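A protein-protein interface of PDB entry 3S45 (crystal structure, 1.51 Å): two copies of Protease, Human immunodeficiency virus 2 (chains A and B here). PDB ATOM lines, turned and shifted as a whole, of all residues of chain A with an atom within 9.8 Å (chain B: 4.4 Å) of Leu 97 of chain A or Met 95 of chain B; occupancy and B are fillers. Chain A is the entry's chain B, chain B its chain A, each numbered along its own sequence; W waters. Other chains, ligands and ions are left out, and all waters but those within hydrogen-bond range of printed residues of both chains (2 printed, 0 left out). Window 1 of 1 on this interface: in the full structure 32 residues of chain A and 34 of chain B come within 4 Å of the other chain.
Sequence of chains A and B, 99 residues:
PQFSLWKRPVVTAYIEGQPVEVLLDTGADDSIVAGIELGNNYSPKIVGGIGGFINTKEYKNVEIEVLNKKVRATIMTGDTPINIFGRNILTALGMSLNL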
ATOM      1  N   PRO A   1      30.472   1.348   5.332  1.00  0.00           N
ATOM      2  CA  PRO A   1      29.053   1.697   5.312  1.00  0.00           C
ATOM      3  C   PRO A   1      28.819   3.157   5.678  1.00  0.00           C
ATOM      4  O   PRO A   1      29.266   3.538   6.754  1.00  0.00           O
ATOM      5  CB  PRO A   1      28.436   0.856   6.428  1.00  0.00           C
ATOM      6  CG  PRO A   1      29.558   0.136   7.081  1.00  0.00           C
ATOM      7  CD  PRO A   1      30.722   0.141   6.137  1.00  0.00           C
ATOM      8  N   GLN A   2      28.129   3.900   4.821  1.00  0.00           N
ATOM      9  CA  GLN A   2      27.780   5.263   5.174  1.00  0.00           C
ATOM     10  C   GLN A   2      26.293   5.409   5.487  1.00  0.00           C
ATOM     11  O   GLN A   2      25.428   4.939   4.751  1.00  0.00           O
ATOM     12  CB  GLN A   2      28.133   6.285   4.075  1.00  0.00           C
ATOM     13  CG  GLN A   2      27.566   7.660   4.405  1.00  0.00           C
ATOM     14  CD  GLN A   2      28.075   8.855   3.638  1.00  0.00           C
ATOM     15  OE1 GLN A   2      29.279   9.066   3.448  1.00  0.00           O
ATOM     16  NE2 GLN A   2      27.154   9.714   3.178  1.00  0.00           N
ATOM     17  N   PHE A   3      26.014   6.098   6.580  1.00  0.00           N
ATOM     18  CA  PHE A   3      24.671   6.541   6.928  1.00  0.00           C
ATOM     19  C   PHE A   3      24.579   8.057   6.719  1.00  0.00           C
ATOM     20  O   PHE A   3      25.294   8.790   7.402  1.00  0.00           O
ATOM     21  CB  PHE A   3      24.370   6.166   8.381  1.00  0.00           C
ATOM     22  CG  PHE A   3      24.329   4.643   8.515  1.00  0.00           C
ATOM     23  CD1 PHE A   3      25.463   3.924   8.843  1.00  0.00           C
ATOM     24  CD2 PHE A   3      23.139   3.970   8.286  1.00  0.00           C
ATOM     25  CE1 PHE A   3      25.431   2.540   8.952  1.00  0.00           C
ATOM     26  CE2 PHE A   3      23.103   2.592   8.393  1.00  0.00           C
ATOM     27  CZ  PHE A   3      24.244   1.872   8.712  1.00  0.00           C
ATOM     28  N   SER A   4      23.728   8.523   5.815  1.00  0.00           N
ATOM     29  CA  SER A   4      23.593   9.932   5.455  1.00  0.00           C
ATOM     30  C   SER A   4      22.639  10.738   6.339  1.00  0.00           C
ATOM     31  O   SER A   4      22.605  11.964   6.232  1.00  0.00           O
ATOM     32  CB  SER A   4      23.144  10.009   3.984  1.00  0.00           C
ATOM     33  OG  SER A   4      24.306   9.840   3.175  1.00  0.00           O
ATOM     34  N   LEU A   5      21.911  10.035   7.182  1.00  0.00           N
ATOM     35  CA  LEU A   5      21.100  10.530   8.293  1.00  0.00           C
ATOM     36  C   LEU A   5      19.818  11.204   7.830  1.00  0.00           C
ATOM     37  O   LEU A   5      19.046  11.744   8.632  1.00  0.00           O
ATOM     38  CB  LEU A   5      21.913  11.446   9.223  1.00  0.00           C
ATOM     39  CG  LEU A   5      23.187  10.815   9.797  1.00  0.00           C
ATOM     40  CD1 LEU A   5      23.983  11.857  10.589  1.00  0.00           C
ATOM     41  CD2 LEU A   5      22.889   9.628  10.685  1.00  0.00           C
ATOM     42  N   TRP A   6      19.567  11.132   6.516  1.00  0.00           N
ATOM     43  CA  TRP A   6      18.245  11.591   6.096  1.00  0.00           C
ATOM     44  C   TRP A   6      17.155  10.638   6.567  1.00  0.00           C
ATOM     45  O   TRP A   6      15.998  11.028   6.743  1.00  0.00           O
ATOM     46  CB  TRP A   6      18.217  11.720   4.584  1.00  0.00           C
ATOM     47  CG  TRP A   6      19.138  12.829   4.143  1.00  0.00           C
ATOM     48  CD1 TRP A   6      20.397  12.721   3.640  1.00  0.00           C
ATOM     49  CD2 TRP A   6      18.824  14.234   4.192  1.00  0.00           C
ATOM     50  NE1 TRP A   6      20.889  13.983   3.362  1.00  0.00           N
ATOM     51  CE2 TRP A   6      19.948  14.920   3.691  1.00  0.00           C
ATOM     52  CE3 TRP A   6      17.698  14.969   4.604  1.00  0.00           C
ATOM     53  CZ2 TRP A   6      19.974  16.315   3.597  1.00  0.00           C
ATOM     54  CZ3 TRP A   6      17.730  16.356   4.510  1.00  0.00           C
ATOM     55  CH2 TRP A   6      18.862  17.014   4.009  1.00  0.00           C
ATOM     56  N   LYS A   7      17.501   9.373   6.767  1.00  0.00           N
ATOM     57  CA  LYS A   7      16.610   8.406   7.407  1.00  0.00           C
ATOM     58  C   LYS A   7      17.293   7.909   8.672  1.00  0.00           C
ATOM     59  O   LYS A   7      18.523   8.085   8.798  1.00  0.00           O
ATOM     60  CB  LYS A   7      16.266   7.278   6.439  1.00  0.00           C
ATOM     61  CG  LYS A   7      17.443   6.429   6.009  1.00  0.00           C
ATOM     62  CD  LYS A   7      17.039   5.214   5.179  1.00  0.00           C
ATOM     63  CE  LYS A   7      18.264   4.419   4.747  1.00  0.00           C
ATOM     64  NZ  LYS A   7      17.906   3.261   3.859  1.00  0.00           N
ATOM     65  N   PRO A   9      19.416   5.762  11.080  1.00  0.00           N
ATOM     66  CA  PRO A   9      20.461   4.754  10.829  1.00  0.00           C
ATOM     67  C   PRO A   9      20.154   3.491  11.622  1.00  0.00           C
ATOM     68  O   PRO A   9      20.727   3.145  12.637  1.00  0.00           O
ATOM     69  CB  PRO A   9      21.727   5.475  11.314  1.00  0.00           C
ATOM     70  CG  PRO A   9      21.255   6.370  12.413  1.00  0.00           C
ATOM     71  CD  PRO A   9      19.847   6.778  12.057  1.00  0.00           C
ATOM     72  N   LEU A  24      21.663   3.082  15.419  1.00  0.00           N
ATOM     73  CA  LEU A  24      23.034   3.497  15.694  1.00  0.00           C
ATOM     74  C   LEU A  24      22.966   4.919  16.241  1.00  0.00           C
ATOM     75  O   LEU A  24      22.659   5.846  15.496  1.00  0.00           O
ATOM     76  CB  LEU A  24      23.881   3.387  14.437  1.00  0.00           C
ATOM     77  CG  LEU A  24      23.855   2.031  13.722  1.00  0.00           C
ATOM     78  CD1 LEU A  24      24.655   2.098  12.427  1.00  0.00           C
ATOM     79  CD2 LEU A  24      24.381   0.913  14.603  1.00  0.00           C
ATOM     80  N   ASP A  25      23.244   5.062  17.522  1.00  0.00           N
ATOM     81  CA  ASP A  25      22.977   6.252  18.330  1.00  0.00           C
ATOM     82  C   ASP A  25      24.191   6.879  18.980  1.00  0.00           C
ATOM     83  O   ASP A  25      24.656   6.459  20.055  1.00  0.00           O
ATOM     84  CB  ASP A  25      22.017   5.792  19.436  1.00  0.00           C
ATOM     85  CG  ASP A  25      21.477   6.989  20.178  1.00  0.00           C
ATOM     86  OD1 ASP A  25      21.836   8.129  19.836  1.00  0.00           O
ATOM     87  OD2 ASP A  25      20.682   6.766  21.107  1.00  0.00           O
ATOM     88  N   THR A  26      24.746   7.923  18.362  1.00  0.00           N
ATOM     89  CA  THR A  26      25.935   8.569  18.916  1.00  0.00           C
ATOM     90  C   THR A  26      25.636   9.303  20.220  1.00  0.00           C
ATOM     91  O   THR A  26      26.610   9.579  20.908  1.00  0.00           O
ATOM     92  CB  THR A  26      26.575   9.573  17.947  1.00  0.00           C
ATOM     93  OG1 THR A  26      25.607  10.534  17.530  1.00  0.00           O
ATOM     94  CG2 THR A  26      27.024   8.835  16.699  1.00  0.00           C
ATOM     95  N   GLY A  27      24.367   9.572  20.489  1.00  0.00           N
ATOM     96  CA  GLY A  27      23.911  10.212  21.720  1.00  0.00           C
ATOM     97  C   GLY A  27      23.734   9.293  22.914  1.00  0.00           C
ATOM     98  O   GLY A  27      23.377   9.770  24.025  1.00  0.00           O
ATOM     99  N   ARG A  87      27.802   4.300  22.039  1.00  0.00           N
ATOM    100  CA  ARG A  87      29.204   4.519  21.693  1.00  0.00           C
ATOM    101  C   ARG A  87      30.075   3.346  22.099  1.00  0.00           C
ATOM    102  O   ARG A  87      31.131   3.141  21.463  1.00  0.00           O
ATOM    103  CB  ARG A  87      29.717   5.825  22.331  1.00  0.00           C
ATOM    104  CG  ARG A  87      29.099   7.058  21.692  1.00  0.00           C
ATOM    105  CD  ARG A  87      29.662   8.396  22.187  1.00  0.00           C
ATOM    106  NE  ARG A  87      29.531   8.486  23.642  1.00  0.00           N
ATOM    107  CZ  ARG A  87      30.443   8.245  24.567  1.00  0.00           C
ATOM    108  NH1 ARG A  87      31.668   7.892  24.230  1.00  0.00           N
ATOM    109  NH2 ARG A  87      30.115   8.369  25.854  1.00  0.00           N
ATOM    110  N   LEU A  90      29.729   1.452  18.984  1.00  0.00           N
ATOM    111  CA  LEU A  90      30.185   2.181  17.795  1.00  0.00           C
ATOM    112  C   LEU A  90      31.705   2.275  17.762  1.00  0.00           C
ATOM    113  O   LEU A  90      32.300   2.083  16.702  1.00  0.00           O
ATOM    114  CB  LEU A  90      29.539   3.569  17.700  1.00  0.00           C
ATOM    115  CG  LEU A  90      28.011   3.554  17.683  1.00  0.00           C
ATOM    116  CD1 LEU A  90      27.475   4.973  17.533  1.00  0.00           C
ATOM    117  CD2 LEU A  90      27.429   2.657  16.594  1.00  0.00           C
ATOM    118  N   THR A  91      32.317   2.548  18.915  1.00  0.00           N
ATOM    119  CA  THR A  91      33.789   2.594  18.901  1.00  0.00           C
ATOM    120  C   THR A  91      34.407   1.212  18.669  1.00  0.00           C
ATOM    121  O   THR A  91      35.498   1.081  18.087  1.00  0.00           O
ATOM    122  CB  THR A  91      34.396   3.152  20.203  1.00  0.00           C
ATOM    123  OG1 THR A  91      33.875   2.372  21.297  1.00  0.00           O
ATOM    124  CG2 THR A  91      34.015   4.604  20.428  1.00  0.00           C
ATOM    125  N   GLY A  94      34.551   0.793  15.032  1.00  0.00           N
ATOM    126  CA  GLY A  94      35.361   1.782  14.358  1.00  0.00           C
ATOM    127  C   GLY A  94      34.581   2.857  13.641  1.00  0.00           C
ATOM    128  O   GLY A  94      35.028   3.413  12.635  1.00  0.00           O
ATOM    129  N   MET A  95      33.390   3.203  14.114  1.00  0.00           N
ATOM    130  CA  MET A  95      32.560   4.187  13.430  1.00  0.00           C
ATOM    131  C   MET A  95      32.929   5.600  13.874  1.00  0.00           C
ATOM    132  O   MET A  95      33.494   5.722  14.964  1.00  0.00           O
ATOM    133  CB  MET A  95      31.073   3.940  13.696  1.00  0.00           C
ATOM    134  CG  MET A  95      30.573   2.560  13.307  1.00  0.00           C
ATOM    135  SD  MET A  95      28.785   2.526  13.038  1.00  0.00           S
ATOM    136  CE  MET A  95      28.690   3.264  11.401  1.00  0.00           C
ATOM    137  N   SER A  96      32.632   6.588  13.045  1.00  0.00           N
ATOM    138  CA  SER A  96      32.853   8.010  13.306  1.00  0.00           C
ATOM    139  C   SER A  96      31.736   8.852  12.682  1.00  0.00           C
ATOM    140  O   SER A  96      31.045   8.363  11.783  1.00  0.00           O
ATOM    141  CB  SER A  96      34.205   8.492  12.782  1.00  0.00           C
ATOM    142  OG  SER A  96      34.244   8.457  11.362  1.00  0.00           O
ATOM    143  N   LEU A  97      31.540  10.062  13.160  1.00  0.00           N
ATOM    144  CA  LEU A  97      30.736  11.154  12.655  1.00  0.00           C
ATOM    145  C   LEU A  97      31.658  12.075  11.843  1.00  0.00           C
ATOM    146  O   LEU A  97      32.727  12.477  12.322  1.00  0.00           O
ATOM    147  CB  LEU A  97      30.112  11.978  13.755  1.00  0.00           C
ATOM    148  CG  LEU A  97      28.678  12.452  13.792  1.00  0.00           C
ATOM    149  CD1 LEU A  97      27.714  11.460  13.160  1.00  0.00           C
ATOM    150  CD2 LEU A  97      28.316  12.761  15.249  1.00  0.00           C
ATOM    151  N   ASN A  98      31.254  12.400  10.627  1.00  0.00           N
ATOM    152  CA  ASN A  98      32.105  13.213   9.767  1.00  0.00           C
ATOM    153  C   ASN A  98      31.323  14.333   9.095  1.00  0.00           C
ATOM    154  O   ASN A  98      30.153  14.148   8.735  1.00  0.00           O
ATOM    155  CB  ASN A  98      32.753  12.319   8.698  1.00  0.00           C
ATOM    156  CG  ASN A  98      33.597  11.224   9.319  1.00  0.00           C
ATOM    157  OD1 ASN A  98      33.122  10.110   9.577  1.00  0.00           O
ATOM    158  ND2 ASN A  98      34.849  11.556   9.581  1.00  0.00           N
ATOM    159  N   LEU A  99      32.001  15.450   8.922  1.00  0.00           N
ATOM    160  CA  LEU A  99      31.555  16.651   8.249  1.00  0.00           C
ATOM    161  C   LEU A  99      32.687  17.163   7.350  1.00  0.00           C
ATOM    162  O   LEU A  99      33.848  16.803   7.618  1.00  0.00           O
ATOM    163  CB  LEU A  99      31.179  17.733   9.245  1.00  0.00           C
ATOM    164  CG  LEU A  99      30.089  18.748   8.921  1.00  0.00           C
ATOM    165  CD1 LEU A  99      30.117  19.886   9.948  1.00  0.00           C
ATOM    166  CD2 LEU A  99      30.208  19.322   7.519  1.00  0.00           C
ATOM    167  OXT LEU A  99      32.382  17.922   6.404  1.00  0.00           O
ATOM    168  N   PRO B   1      35.982  17.923  10.029  1.00  0.00           N
ATOM    169  CA  PRO B   1      35.479  17.550  11.348  1.00  0.00           C
ATOM    170  C   PRO B   1      35.139  16.063  11.400  1.00  0.00           C
ATOM    171  O   PRO B   1      34.314  15.605  10.612  1.00  0.00           O
ATOM    172  CB  PRO B   1      34.182  18.351  11.499  1.00  0.00           C
ATOM    173  CG  PRO B   1      34.387  19.530  10.604  1.00  0.00           C
ATOM    174  CD  PRO B   1      35.193  19.021   9.440  1.00  0.00           C
ATOM    175  N   GLN B   2      35.789  15.385  12.327  1.00  0.00           N
ATOM    176  CA  GLN B   2      35.522  13.968  12.558  1.00  0.00           C
ATOM    177  C   GLN B   2      35.428  13.690  14.046  1.00  0.00           C
ATOM    178  O   GLN B   2      36.327  14.051  14.822  1.00  0.00           O
ATOM    179  CB  GLN B   2      36.626  13.136  11.898  1.00  0.00           C
ATOM    180  CG  GLN B   2      36.596  11.665  12.290  1.00  0.00           C
ATOM    181  CD  GLN B   2      37.418  10.803  11.348  1.00  0.00           C
ATOM    182  OE1 GLN B   2      37.009  10.479  10.227  1.00  0.00           O
ATOM    183  NE2 GLN B   2      38.606  10.419  11.811  1.00  0.00           N
ATOM    184  N   PHE B   3      34.354  13.066  14.469  1.00  0.00           N
ATOM    185  CA  PHE B   3      34.176  12.714  15.882  1.00  0.00           C
ATOM    186  C   PHE B   3      34.304  11.208  16.079  1.00  0.00           C
ATOM    187  O   PHE B   3      33.477  10.455  15.551  1.00  0.00           O
ATOM    188  CB  PHE B   3      32.799  13.189  16.352  1.00  0.00           C
ATOM    189  CG  PHE B   3      32.649  14.699  16.250  1.00  0.00           C
ATOM    190  CD1 PHE B   3      32.301  15.291  15.048  1.00  0.00           C
ATOM    191  CD2 PHE B   3      32.870  15.489  17.364  1.00  0.00           C
ATOM    192  CE1 PHE B   3      32.192  16.662  14.937  1.00  0.00           C
ATOM    193  CE2 PHE B   3      32.779  16.865  17.259  1.00  0.00           C
ATOM    194  CZ  PHE B   3      32.462  17.442  16.045  1.00  0.00           C
ATOM    195  N   LEU B  24      25.704  15.862  19.538  1.00  0.00           N
ATOM    196  CA  LEU B  24      25.392  15.525  18.147  1.00  0.00           C
ATOM    197  C   LEU B  24      24.868  14.102  18.110  1.00  0.00           C
ATOM    198  O   LEU B  24      25.643  13.166  18.322  1.00  0.00           O
ATOM    199  CB  LEU B  24      26.617  15.661  17.257  1.00  0.00           C
ATOM    200  CG  LEU B  24      27.391  16.983  17.336  1.00  0.00           C
ATOM    201  CD1 LEU B  24      28.649  16.898  16.477  1.00  0.00           C
ATOM    202  CD2 LEU B  24      26.482  18.122  16.911  1.00  0.00           C
ATOM    203  N   THR B  26      22.856  10.900  16.468  1.00  0.00           N
ATOM    204  CA  THR B  26      22.234  10.250  15.303  1.00  0.00           C
ATOM    205  C   THR B  26      20.984   9.481  15.680  1.00  0.00           C
ATOM    206  O   THR B  26      20.195   9.103  14.811  1.00  0.00           O
ATOM    207  CB  THR B  26      23.223   9.300  14.597  1.00  0.00           C
ATOM    208  OG1 THR B  26      23.669   8.338  15.571  1.00  0.00           O
ATOM    209  CG2 THR B  26      24.432  10.060  14.067  1.00  0.00           C
ATOM    210  N   LEU B  67      29.572  24.258  14.303  1.00  0.00           N
ATOM    211  CA  LEU B  67      30.632  23.740  13.451  1.00  0.00           C
ATOM    212  C   LEU B  67      30.916  24.701  12.302  1.00  0.00           C
ATOM    213  O   LEU B  67      30.938  24.298  11.135  1.00  0.00           O
ATOM    214  CB  LEU B  67      30.278  22.358  12.905  1.00  0.00           C
ATOM    215  CG  LEU B  67      30.605  21.222  13.883  1.00  0.00           C
ATOM    216  CD1 LEU B  67      29.423  20.921  14.787  1.00  0.00           C
ATOM    217  CD2 LEU B  67      31.024  19.976  13.117  1.00  0.00           C
ATOM    218  N   LEU B  90      21.830  17.608  11.816  1.00  0.00           N
ATOM    219  CA  LEU B  90      23.008  16.945  11.264  1.00  0.00           C
ATOM    220  C   LEU B  90      22.974  16.850   9.749  1.00  0.00           C
ATOM    221  O   LEU B  90      24.001  17.033   9.103  1.00  0.00           O
ATOM    222  CB  LEU B  90      23.167  15.530  11.842  1.00  0.00           C
ATOM    223  CG  LEU B  90      23.187  15.483  13.370  1.00  0.00           C
ATOM    224  CD1 LEU B  90      23.469  14.080  13.873  1.00  0.00           C
ATOM    225  CD2 LEU B  90      24.216  16.459  13.919  1.00  0.00           C
ATOM    226  N   LEU B  93      23.681  20.146   8.106  1.00  0.00           N
ATOM    227  CA  LEU B  93      25.112  20.419   8.164  1.00  0.00           C
ATOM    228  C   LEU B  93      25.885  19.524   7.197  1.00  0.00           C
ATOM    229  O   LEU B  93      27.077  19.768   6.963  1.00  0.00           O
ATOM    230  CB  LEU B  93      25.620  20.217   9.589  1.00  0.00           C
ATOM    231  CG  LEU B  93      25.010  21.114  10.667  1.00  0.00           C
ATOM    232  CD1 LEU B  93      25.417  20.650  12.049  1.00  0.00           C
ATOM    233  CD2 LEU B  93      25.444  22.560  10.481  1.00  0.00           C
ATOM    234  N   GLY B  94      25.247  18.490   6.639  1.00  0.00           N
ATOM    235  CA  GLY B  94      25.954  17.576   5.744  1.00  0.00           C
ATOM    236  C   GLY B  94      26.782  16.530   6.476  1.00  0.00           C
ATOM    237  O   GLY B  94      27.740  16.018   5.878  1.00  0.00           O
ATOM    238  N   MET B  95      26.444  16.209   7.725  1.00  0.00           N
ATOM    239  CA  MET B  95      27.178  15.220   8.515  1.00  0.00           C
ATOM    240  C   MET B  95      26.795  13.793   8.117  1.00  0.00           C
ATOM    241  O   MET B  95      25.681  13.533   7.664  1.00  0.00           O
ATOM    242  CB  MET B  95      26.934  15.428  10.014  1.00  0.00           C
ATOM    243  CG  MET B  95      27.911  14.759  10.960  1.00  0.00           C
ATOM    244  SD  MET B  95      27.858  15.364  12.664  1.00  0.00           S
ATOM    245  CE  MET B  95      28.729  16.921  12.502  1.00  0.00           C
ATOM    246  N   SER B  96      27.717  12.855   8.300  1.00  0.00           N
ATOM    247  CA  SER B  96      27.394  11.456   8.005  1.00  0.00           C
ATOM    248  C   SER B  96      27.951  10.579   9.122  1.00  0.00           C
ATOM    249  O   SER B  96      28.874  10.981   9.836  1.00  0.00           O
ATOM    250  CB  SER B  96      27.990  11.070   6.655  1.00  0.00           C
ATOM    251  OG  SER B  96      29.410  11.157   6.675  1.00  0.00           O
ATOM    252  N   LEU B  97      27.390   9.399   9.254  1.00  0.00           N
ATOM    253  CA  LEU B  97      27.866   8.378  10.173  1.00  0.00           C
ATOM    254  C   LEU B  97      28.495   7.266   9.341  1.00  0.00           C
ATOM    255  O   LEU B  97      27.862   6.691   8.457  1.00  0.00           O
ATOM    256  CB  LEU B  97      26.728   7.856  11.029  1.00  0.00           C
ATOM    257  CG  LEU B  97      27.030   6.760  12.042  1.00  0.00           C
ATOM    258  CD1 LEU B  97      28.031   7.221  13.104  1.00  0.00           C
ATOM    259  CD2 LEU B  97      25.704   6.305  12.644  1.00  0.00           C
HETATM  260  O   HOH W   1      29.769  13.656   5.345  1.00  0.00           O
HETATM  261  O   HOH W   2      24.006  13.974   5.829  1.00  0.00           O
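The side-chain amide nitrogen of Asn 98 of chain A is in hydrogen-bond range of the side-chain amide oxygen of Gln 2 of chain B (2.5 Å).
O of Leu 24 of chain A sits at hydrogen-bond distance from OG1 of Thr 26 of chain B, 2.7 Å away.
The side-chain hydroxyl (OG1) of Thr 26 of chain A lies within hydrogen-bond range of the backbone carbonyl oxygen (O) of Leu 24 of chain B (2.7 Å).
The backbone NH of Ser 96 of chain B sits at hydrogen-bond distance from the backbone carbonyl oxygen of Asn 98 of chain A (2.8 Å).
The backbone NH of Thr 26 of chain B is in hydrogen-bond range of the side-chain hydroxyl of Thr 26 of chain A (3.0 Å).
The backbone NH of Phe 3 of chain B sits at hydrogen-bond distance from the backbone carbonyl oxygen of Leu 97 of chain A (2.8 Å).
The backbone carbonyl oxygen (O) of Pro 1 of chain B is in hydrogen-bond range of the backbone NH (N) of Leu 99 of chain A, 2.9 Å away.
N of Phe 3 of chain A is in hydrogen-bond range of O of Leu 97 of chain B (2.7 Å).
The side-chain carboxylate (OD1) of Asp 25 of chain A sits at hydrogen-bond distance from the backbone NH (N) of Gly 27 of chain A (3.0 Å).
The side-chain amide nitrogen of Gln 2 of chain A lies within hydrogen-bond range of the side-chain hydroxyl of Ser 4 of chain A (2.9 Å).
O of Leu 90 of chain B is in hydrogen-bond range of N of Met 95 of chain B (2.9 Å).
N of Met 95 of chain A is in hydrogen-bond range of O of Leu 90 of chain A, at 3.0 Å.
The backbone carbonyl oxygen (O) of Pro 9 of chain A sits at hydrogen-bond distance from the backbone NH (N) of Leu 24 of chain A (2.9 Å).
The side-chain hydroxyl (OG) of Ser 96 of chain A sits at hydrogen-bond distance from the side-chain amide oxygen (OD1) of Asn 98 of chain A (2.7 Å).
Leu 97 of chain B touches Pro 1 of chain A (O to O, 3.8 Å).
Ser 96 of chain B touches Phe 3 of chain A (CA to O, 3.4 Å).
O of Met 95 of chain B touches O of Ser 4 of chain A, 3.7 Å away.
Leu 90 of chain B touches Leu 5 of chain A (CB to CD1, 3.97 Å).
CD1 of Leu 5 of chain A touches O of Met 95 of chain B (3.8 Å).
Leu 97 of chain B touches Leu 24 of chain A (CD2 to CB, 3.9 Å).
CA of Asp 25 of chain A touches OG1 of Thr 26 of chain B, at 3.5 Å.
Phe 3 of chain B touches Ser 96 of chain A.
Ser 96 of chain A touches Leu 97 of chain B.
Pro 1 of chain B touches Leu 97 of chain A (O to O, 3.9 Å).
Of the printed residues of chain B, Gln 2 of chain A touches Ser 96 (3.7 Å) and Leu 97 (3.6 Å).
Of the printed residues of chain B, Asp 25 of chain A touches Thr 26 (3.5 Å).
Leu 90 of chain A touches none of the printed residues of chain B.
Of the printed residues of chain B, Leu 97 of chain A touches Pro 1 (3.9 Å), Gln 2 (3.2 Å), Phe 3 (2.8 Å), Leu 24 (3.9 Å), Thr 26 (3.7 Å), Met 95 (3.2 Å) and Ser 96 (3.4 Å).
Of the printed residues of chain B, Leu 99 of chain A touches Pro 1 (2.9 Å), Leu 67 (3.3 Å) and Leu 93 (3.2 Å).
Of the printed residues of chain A, Leu 24 of chain B touches Thr 26 (2.7 Å) and Leu 97 (3.9 Å).
Of the printed residues of chain A, Met 95 of chain B touches Ser 4, Leu 5, Leu 97 and Asn 98.
Ser 96 of chain B touches five residues of chain A.
The nearest printed residue of chain B that does not touch Leu 97 of chain A is Leu 97 of chain B (4.3 Å).
The nearest printed residue of chain A that does not touch Met 95 of chain B is Leu 99 of chain A (4.2 Å).
Printed residues of chain B that touch a printed residue of chain A: Pro 1, Gln 2, Phe 3, Leu 24, Thr 26, Leu 67, Leu 90, Leu 93, Met 95, Ser 96 and Leu 97.
Hydrophobic or aromatic side chains of chain B that line the printed part of chain A: Pro 1, Phe 3, Leu 24, Leu 67, Leu 90, Met 95 and Leu 97.
Among the printed residues, 34 pairs touch across the chains.
Phe 3 of chain A touches Ser 96 of chain B, and with the chains exchanged Ser 96 of chain A touches Phe 3 of chain B.
Leu 24 of chain A touches Thr 26 of chain B, and with the chains exchanged Thr 26 of chain A touches Leu 24 of chain B.
Thr 26 of chain A touches its own counterpart, Thr 26 of chain B.
Ser 96 of chain A touches its own counterpart, Ser 96 of chain B.
Water W2 lies within hydrogen-bond range of the backbone carbonyl oxygen of Ser 4 of chain A and the backbone carbonyl oxygen of Met 95 of chain B.
Water W1 lies within hydrogen-bond range of OG of Ser 96 of chain B, O of Gly 94 of chain B and O of Asn 98 of chain A.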
